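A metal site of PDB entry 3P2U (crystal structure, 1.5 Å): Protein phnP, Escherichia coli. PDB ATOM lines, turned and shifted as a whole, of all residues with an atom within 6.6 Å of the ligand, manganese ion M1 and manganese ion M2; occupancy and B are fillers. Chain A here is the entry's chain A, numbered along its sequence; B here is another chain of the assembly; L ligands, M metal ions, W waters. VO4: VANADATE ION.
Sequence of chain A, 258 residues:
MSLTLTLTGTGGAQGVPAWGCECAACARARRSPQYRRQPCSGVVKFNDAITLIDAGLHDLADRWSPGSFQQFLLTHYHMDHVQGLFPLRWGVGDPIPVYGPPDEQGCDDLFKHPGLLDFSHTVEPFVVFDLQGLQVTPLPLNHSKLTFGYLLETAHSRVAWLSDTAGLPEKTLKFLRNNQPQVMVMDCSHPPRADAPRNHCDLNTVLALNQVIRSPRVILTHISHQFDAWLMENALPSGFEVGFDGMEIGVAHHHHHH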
ATOM      1  N   GLY A  11      19.468  -8.431  21.705  1.00  0.00           N
ATOM      2  CA  GLY A  11      20.163  -9.571  21.130  1.00  0.00           C
ATOM      3  C   GLY A  11      19.231 -10.573  20.483  1.00  0.00           C
ATOM      4  O   GLY A  11      18.018 -10.421  20.485  1.00  0.00           O
ATOM      5  N   GLY A  12      19.820 -11.619  19.916  1.00  0.00           N
ATOM      6  CA  GLY A  12      19.038 -12.757  19.466  1.00  0.00           C
ATOM      7  C   GLY A  12      19.068 -13.862  20.493  1.00  0.00           C
ATOM      8  O   GLY A  12      19.470 -13.658  21.643  1.00  0.00           O
ATOM      9  N   ALA A  13      18.628 -15.037  20.089  1.00  0.00           N
ATOM     10  CA  ALA A  13      18.528 -16.168  20.995  1.00  0.00           C
ATOM     11  C   ALA A  13      19.853 -16.517  21.687  1.00  0.00           C
ATOM     12  O   ALA A  13      19.904 -16.858  22.874  1.00  0.00           O
ATOM     13  CB  ALA A  13      17.993 -17.381  20.246  1.00  0.00           C
ATOM     14  N   GLN A  14      20.940 -16.420  20.928  1.00  0.00           N
ATOM     15  CA  GLN A  14      22.275 -16.744  21.416  1.00  0.00           C
ATOM     16  C   GLN A  14      22.777 -15.738  22.447  1.00  0.00           C
ATOM     17  O   GLN A  14      23.528 -16.081  23.357  1.00  0.00           O
ATOM     18  CB  GLN A  14      23.212 -16.811  20.223  1.00  0.00           C
ATOM     19  CG  GLN A  14      24.690 -17.050  20.527  1.00  0.00           C
ATOM     20  CD  GLN A  14      25.499 -17.080  19.246  1.00  0.00           C
ATOM     21  OE1 GLN A  14      25.504 -16.099  18.487  1.00  0.00           O
ATOM     22  NE2 GLN A  14      26.152 -18.197  18.965  1.00  0.00           N
ATOM     23  N   CYS A  40      15.593 -10.029  22.253  1.00  0.00           N
ATOM     24  CA  CYS A  40      14.916  -8.909  21.623  1.00  0.00           C
ATOM     25  C   CYS A  40      13.504  -8.682  22.157  1.00  0.00           C
ATOM     26  O   CYS A  40      12.606  -9.488  21.931  1.00  0.00           O
ATOM     27  CB  CYS A  40      14.860  -9.154  20.119  1.00  0.00           C
ATOM     28  SG  CYS A  40      14.199  -7.779  19.175  1.00  0.00           S
ATOM     29  N   HIS A  76       5.973 -13.327  17.609  1.00  0.00           N
ATOM     30  CA  HIS A  76       5.921 -14.718  17.196  1.00  0.00           C
ATOM     31  C   HIS A  76       6.295 -15.609  18.359  1.00  0.00           C
ATOM     32  O   HIS A  76       6.693 -15.108  19.408  1.00  0.00           O
ATOM     33  CB  HIS A  76       6.804 -15.003  15.961  1.00  0.00           C
ATOM     34  CG  HIS A  76       8.283 -14.875  16.190  1.00  0.00           C
ATOM     35  ND1 HIS A  76       8.882 -13.709  16.646  1.00  0.00           N
ATOM     36  CD2 HIS A  76       9.306 -15.724  15.904  1.00  0.00           C
ATOM     37  CE1 HIS A  76      10.198 -13.861  16.655  1.00  0.00           C
ATOM     38  NE2 HIS A  76      10.475 -15.073  16.202  1.00  0.00           N
ATOM     39  N   HIS A  78       8.607 -18.174  18.647  1.00  0.00           N
ATOM     40  CA  HIS A  78       9.930 -18.735  18.914  1.00  0.00           C
ATOM     41  C   HIS A  78      10.254 -18.582  20.397  1.00  0.00           C
ATOM     42  O   HIS A  78       9.855 -17.616  21.059  1.00  0.00           O
ATOM     43  CB  HIS A  78      11.016 -18.066  18.075  1.00  0.00           C
ATOM     44  CG  HIS A  78      11.204 -18.694  16.724  1.00  0.00           C
ATOM     45  ND1 HIS A  78      11.553 -17.969  15.608  1.00  0.00           N
ATOM     46  CD2 HIS A  78      11.077 -19.980  16.320  1.00  0.00           C
ATOM     47  CE1 HIS A  78      11.648 -18.782  14.566  1.00  0.00           C
ATOM     48  NE2 HIS A  78      11.359 -20.005  14.981  1.00  0.00           N
ATOM     49  N   MET A  79      10.999 -19.545  20.928  1.00  0.00           N
ATOM     50  CA  MET A  79      11.254 -19.589  22.357  1.00  0.00           C
ATOM     51  C   MET A  79      11.877 -18.330  22.921  1.00  0.00           C
ATOM     52  O   MET A  79      11.524 -17.914  24.025  1.00  0.00           O
ATOM     53  CB  MET A  79      12.130 -20.800  22.703  1.00  0.00           C
ATOM     54  CG  MET A  79      12.291 -21.046  24.205  1.00  0.00           C
ATOM     55  SD  MET A  79      10.719 -21.376  25.069  1.00  0.00           S
ATOM     56  CE  MET A  79      10.481 -23.092  24.611  1.00  0.00           C
ATOM     57  N   ASP A  80      12.800 -17.719  22.168  1.00  0.00           N
ATOM     58  CA  ASP A  80      13.500 -16.529  22.663  1.00  0.00           C
ATOM     59  C   ASP A  80      12.603 -15.296  22.713  1.00  0.00           C
ATOM     60  O   ASP A  80      13.041 -14.235  23.147  1.00  0.00           O
ATOM     61  CB  ASP A  80      14.803 -16.240  21.887  1.00  0.00           C
ATOM     62  CG  ASP A  80      14.590 -16.021  20.392  1.00  0.00           C
ATOM     63  OD1 ASP A  80      13.889 -16.825  19.761  1.00  0.00           O
ATOM     64  OD2 ASP A  80      15.118 -15.023  19.843  1.00  0.00           O
ATOM     65  N   HIS A  81      11.351 -15.435  22.263  1.00  0.00           N
ATOM     66  CA  HIS A  81      10.375 -14.349  22.379  1.00  0.00           C
ATOM     67  C   HIS A  81       9.239 -14.641  23.350  1.00  0.00           C
ATOM     68  O   HIS A  81       8.436 -13.741  23.657  1.00  0.00           O
ATOM     69  CB  HIS A  81       9.827 -13.986  20.991  1.00  0.00           C
ATOM     70  CG  HIS A  81      10.886 -13.499  20.054  1.00  0.00           C
ATOM     71  ND1 HIS A  81      11.062 -12.174  19.725  1.00  0.00           N
ATOM     72  CD2 HIS A  81      11.911 -14.167  19.449  1.00  0.00           C
ATOM     73  CE1 HIS A  81      12.100 -12.044  18.917  1.00  0.00           C
ATOM     74  NE2 HIS A  81      12.645 -13.254  18.759  1.00  0.00           N
ATOM     75  N   HIS A 143       9.788 -14.789   7.974  1.00  0.00           N
ATOM     76  CA  HIS A 143      10.408 -15.543   9.062  1.00  0.00           C
ATOM     77  C   HIS A 143       9.882 -16.979   9.065  1.00  0.00           C
ATOM     78  O   HIS A 143       8.834 -17.261   8.482  1.00  0.00           O
ATOM     79  CB  HIS A 143      10.080 -14.864  10.407  1.00  0.00           C
ATOM     80  CG  HIS A 143      11.038 -15.168  11.514  1.00  0.00           C
ATOM     81  ND1 HIS A 143      12.408 -15.002  11.386  1.00  0.00           N
ATOM     82  CD2 HIS A 143      10.829 -15.594  12.785  1.00  0.00           C
ATOM     83  CE1 HIS A 143      12.994 -15.323  12.526  1.00  0.00           C
ATOM     84  NE2 HIS A 143      12.065 -15.688  13.390  1.00  0.00           N
ATOM     85  N   SER A 144      10.590 -17.881   9.732  1.00  0.00           N
ATOM     86  CA  SER A 144      10.244 -19.306   9.680  1.00  0.00           C
ATOM     87  C   SER A 144       8.965 -19.644  10.452  1.00  0.00           C
ATOM     88  O   SER A 144       8.375 -20.711  10.268  1.00  0.00           O
ATOM     89  CB  SER A 144      11.418 -20.155  10.173  1.00  0.00           C
ATOM     90  OG  SER A 144      11.803 -19.764  11.477  1.00  0.00           O
ATOM     91  N   LYS A 145       8.557 -18.747  11.350  1.00  0.00           N
ATOM     92  CA  LYS A 145       7.284 -18.832  12.041  1.00  0.00           C
ATOM     93  C   LYS A 145       6.365 -17.726  11.562  1.00  0.00           C
ATOM     94  O   LYS A 145       6.845 -16.716  11.048  1.00  0.00           O
ATOM     95  CB  LYS A 145       7.482 -18.603  13.539  1.00  0.00           C
ATOM     96  CG  LYS A 145       8.258 -19.681  14.245  1.00  0.00           C
ATOM     97  CD  LYS A 145       7.312 -20.706  14.786  1.00  0.00           C
ATOM     98  CE  LYS A 145       7.978 -21.528  15.862  1.00  0.00           C
ATOM     99  NZ  LYS A 145       7.081 -22.618  16.293  1.00  0.00           N
ATOM    100  N   THR A 147       4.935 -14.527  11.836  1.00  0.00           N
ATOM    101  CA  THR A 147       5.556 -13.453  12.605  1.00  0.00           C
ATOM    102  C   THR A 147       5.006 -12.102  12.165  1.00  0.00           C
ATOM    103  O   THR A 147       4.954 -11.821  10.960  1.00  0.00           O
ATOM    104  CB  THR A 147       7.084 -13.460  12.363  1.00  0.00           C
ATOM    105  OG1 THR A 147       7.607 -14.753  12.713  1.00  0.00           O
ATOM    106  CG2 THR A 147       7.788 -12.374  13.194  1.00  0.00           C
ATOM    107  N   SER A 163      11.019  -7.044  14.149  1.00  0.00           N
ATOM    108  CA  SER A 163      11.868  -8.227  14.360  1.00  0.00           C
ATOM    109  C   SER A 163      10.876  -9.347  14.650  1.00  0.00           C
ATOM    110  O   SER A 163       9.835  -9.076  15.268  1.00  0.00           O
ATOM    111  CB  SER A 163      12.782  -7.974  15.553  1.00  0.00           C
ATOM    112  OG  SER A 163      13.973  -8.761  15.471  1.00  0.00           O
ATOM    113  N   ASP A 164      11.142 -10.593  14.245  1.00  0.00           N
ATOM    114  CA  ASP A 164      12.322 -11.032  13.474  1.00  0.00           C
ATOM    115  C   ASP A 164      11.961 -11.108  12.001  1.00  0.00           C
ATOM    116  O   ASP A 164      10.869 -11.563  11.646  1.00  0.00           O
ATOM    117  CB  ASP A 164      12.675 -12.458  13.869  1.00  0.00           C
ATOM    118  CG  ASP A 164      13.122 -12.603  15.316  1.00  0.00           C
ATOM    119  OD1 ASP A 164      13.216 -11.627  16.090  1.00  0.00           O
ATOM    120  OD2 ASP A 164      13.403 -13.762  15.648  1.00  0.00           O
ATOM    121  N   ASP A 187      15.302  -5.700  12.934  1.00  0.00           N
ATOM    122  CA  ASP A 187      16.189  -6.860  12.983  1.00  0.00           C
ATOM    123  C   ASP A 187      17.381  -6.632  12.077  1.00  0.00           C
ATOM    124  O   ASP A 187      17.227  -6.449  10.869  1.00  0.00           O
ATOM    125  CB  ASP A 187      15.409  -8.070  12.495  1.00  0.00           C
ATOM    126  CG  ASP A 187      16.152  -9.397  12.681  1.00  0.00           C
ATOM    127  OD1 ASP A 187      17.392  -9.417  12.866  1.00  0.00           O
ATOM    128  OD2 ASP A 187      15.477 -10.424  12.631  1.00  0.00           O
ATOM    129  N   SER A 189      20.546  -8.902  12.380  1.00  0.00           N
ATOM    130  CA  SER A 189      21.304  -9.885  13.137  1.00  0.00           C
ATOM    131  C   SER A 189      22.747  -9.918  12.660  1.00  0.00           C
ATOM    132  O   SER A 189      23.658 -10.088  13.465  1.00  0.00           O
ATOM    133  CB  SER A 189      20.673 -11.258  12.963  1.00  0.00           C
ATOM    134  OG  SER A 189      19.387 -11.314  13.560  1.00  0.00           O
ATOM    135  N   ASN A 199      16.538 -15.956   7.564  1.00  0.00           N
ATOM    136  CA  ASN A 199      15.589 -15.781   8.669  1.00  0.00           C
ATOM    137  C   ASN A 199      15.718 -14.393   9.332  1.00  0.00           C
ATOM    138  O   ASN A 199      14.797 -13.929  10.002  1.00  0.00           O
ATOM    139  CB  ASN A 199      15.788 -16.885   9.720  1.00  0.00           C
ATOM    140  CG  ASN A 199      14.466 -17.522  10.195  1.00  0.00           C
ATOM    141  OD1 ASN A 199      14.405 -18.081  11.291  1.00  0.00           O
ATOM    142  ND2 ASN A 199      13.436 -17.462   9.361  1.00  0.00           N
ATOM    143  N   HIS A 200      16.880 -13.766   9.127  1.00  0.00           N
ATOM    144  CA  HIS A 200      17.150 -12.432   9.682  1.00  0.00           C
ATOM    145  C   HIS A 200      17.910 -11.597   8.681  1.00  0.00           C
ATOM    146  O   HIS A 200      18.652 -12.134   7.860  1.00  0.00           O
ATOM    147  CB  HIS A 200      17.999 -12.542  10.953  1.00  0.00           C
ATOM    148  CG  HIS A 200      17.368 -13.355  12.034  1.00  0.00           C
ATOM    149  ND1 HIS A 200      16.413 -12.844  12.892  1.00  0.00           N
ATOM    150  CD2 HIS A 200      17.555 -14.638  12.395  1.00  0.00           C
ATOM    151  CE1 HIS A 200      16.040 -13.796  13.730  1.00  0.00           C
ATOM    152  NE2 HIS A 200      16.715 -14.889  13.458  1.00  0.00           N
ATOM    153  N   HIS A 222      18.275  -7.089  17.602  1.00  0.00           N
ATOM    154  CA  HIS A 222      18.476  -8.531  17.393  1.00  0.00           C
ATOM    155  C   HIS A 222      19.919  -8.803  16.908  1.00  0.00           C
ATOM    156  O   HIS A 222      20.156  -9.654  16.044  1.00  0.00           O
ATOM    157  CB  HIS A 222      17.422  -9.091  16.425  1.00  0.00           C
ATOM    158  CG  HIS A 222      17.076 -10.529  16.664  1.00  0.00           C
ATOM    159  ND1 HIS A 222      17.849 -11.567  16.202  1.00  0.00           N
ATOM    160  CD2 HIS A 222      16.017 -11.110  17.284  1.00  0.00           C
ATOM    161  CE1 HIS A 222      17.295 -12.721  16.536  1.00  0.00           C
ATOM    162  NE2 HIS A 222      16.189 -12.469  17.203  1.00  0.00           N
ATOM    163  N   ARG B  89      22.464 -23.716  24.150  1.00  0.00           N
ATOM    164  CA  ARG B  89      22.730 -24.580  23.008  1.00  0.00           C
ATOM    165  C   ARG B  89      23.479 -23.871  21.878  1.00  0.00           C
ATOM    166  O   ARG B  89      24.157 -24.504  21.075  1.00  0.00           O
ATOM    167  CB  ARG B  89      21.427 -25.195  22.496  1.00  0.00           C
ATOM    168  CG  ARG B  89      20.424 -24.155  22.027  1.00  0.00           C
ATOM    169  CD  ARG B  89      19.122 -24.813  21.596  1.00  0.00           C
ATOM    170  NE  ARG B  89      18.084 -23.806  21.407  1.00  0.00           N
ATOM    171  CZ  ARG B  89      17.000 -23.990  20.674  1.00  0.00           C
ATOM    172  NH1 ARG B  89      16.810 -25.147  20.050  1.00  0.00           N
ATOM    173  NH2 ARG B  89      16.090 -23.021  20.572  1.00  0.00           N
ATOM    174  N   TRP B  90      23.352 -22.539  21.825  1.00  0.00           N
ATOM    175  CA  TRP B  90      23.959 -21.756  20.768  1.00  0.00           C
ATOM    176  C   TRP B  90      25.407 -21.394  21.094  1.00  0.00           C
ATOM    177  O   TRP B  90      26.033 -20.582  20.396  1.00  0.00           O
ATOM    178  CB  TRP B  90      23.137 -20.478  20.542  1.00  0.00           C
ATOM    179  CG  TRP B  90      21.678 -20.695  20.279  1.00  0.00           C
ATOM    180  CD1 TRP B  90      20.632 -20.251  21.020  1.00  0.00           C
ATOM    181  CD2 TRP B  90      21.102 -21.439  19.194  1.00  0.00           C
ATOM    182  NE1 TRP B  90      19.438 -20.661  20.477  1.00  0.00           N
ATOM    183  CE2 TRP B  90      19.708 -21.377  19.342  1.00  0.00           C
ATOM    184  CE3 TRP B  90      21.630 -22.150  18.118  1.00  0.00           C
ATOM    185  CZ2 TRP B  90      18.823 -22.010  18.458  1.00  0.00           C
ATOM    186  CZ3 TRP B  90      20.764 -22.770  17.234  1.00  0.00           C
ATOM    187  CH2 TRP B  90      19.372 -22.697  17.414  1.00  0.00           C
ATOM    188  N   ASP B 109      11.983 -26.814  20.000  1.00  0.00           N
ATOM    189  CA  ASP B 109      12.918 -27.250  18.956  1.00  0.00           C
ATOM    190  C   ASP B 109      14.313 -27.674  19.435  1.00  0.00           C
ATOM    191  O   ASP B 109      15.281 -27.609  18.677  1.00  0.00           O
ATOM    192  CB  ASP B 109      13.021 -26.222  17.828  1.00  0.00           C
ATOM    193  CG  ASP B 109      13.716 -24.951  18.242  1.00  0.00           C
ATOM    194  OD1 ASP B 109      14.036 -24.802  19.434  1.00  0.00           O
ATOM    195  OD2 ASP B 109      13.945 -24.096  17.366  1.00  0.00           O
HETATM  196  V   VO4 L   1      15.700 -16.806  15.878  1.00  0.00           V
HETATM  197  O1  VO4 L   1      14.231 -16.681  14.673  1.00  0.00           O
HETATM  198  O2  VO4 L   1      15.951 -15.226  16.914  1.00  0.00           O
HETATM  199  O3  VO4 L   1      15.427 -18.279  17.052  1.00  0.00           O
HETATM  200  O4  VO4 L   1      17.269 -17.100  14.819  1.00  0.00           O
HETATM  201 MN    MN M   1      14.442 -14.077  17.609  1.00  0.00          MN
HETATM  202 MN    MN M   2      12.343 -15.962  15.481  1.00  0.00          MN
HETATM  203  O   HOH W   1      14.607 -19.591  19.755  1.00  0.00           O
HETATM  204  O   HOH W   2      13.346 -16.097  17.289  1.00  0.00           O
HETATM  205  O   HOH W   3      18.263 -15.761  17.346  1.00  0.00           O
HETATM  206  O   HOH W   4      15.107 -20.387  15.564  1.00  0.00           O
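A ring nitrogen (ND1) of His 143 is in hydrogen-bond range of the backbone carbonyl oxygen of Asn 199, 3.0 Å away.
OD1 of Asp 164 lies within hydrogen-bond range of OG of Ser 163 (3.0 Å).
A ring nitrogen (ND1) of His 222 is in hydrogen-bond range of the side-chain hydroxyl (OG) of Ser 189, at 3.1 Å.
OG of Ser 189 sits close to ND1 of His 200 (3.4 Å).
The side-chain carboxylate (OD2) of Asp 187 is in hydrogen-bond range of a ring nitrogen (ND1) of His 200 (2.6 Å).
The backbone NH of Ser 144 sits close to the side-chain amide nitrogen of Asn 199, at 2.9 Å.
Along chain A the residues within 4 Å of manganese ion M2 span positions 76 to 164.
Manganese ion M1 is bound by O2 of the ligand (2.0 Å), OD2 of Asp 164 (2.2 Å), NE2 of His 81 (2.3 Å), water W2 (2.3 Å), NE2 of His 222 (2.4 Å) and OD2 of Asp 80 (2.5 Å).
Manganese ion M1 has six donor atoms within binding distance.
OD1 of Asn 199 touches O1 of the ligand, at 3.7 Å.
Hydrophobic or aromatic side chains within 4 Å of the ligand: His 78, His 143, His 200 and His 222.
Of the 24 residues printed, 7 come within 4 Å of the ligand.
The nearest printed residue that does not touch the ligand is Ala 13 (4.2 Å).
NE2 of His 200 lies close to O4 of the ligand (2.7 Å).
Manganese ion M2 is bound by water W2 (2.1 Å), NE2 of His 143 (2.1 Å), ND1 of His 78 (2.2 Å), O1 of the ligand (2.2 Å), NE2 of His 76 (2.2 Å) and OD2 of Asp 164 (2.4 Å).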
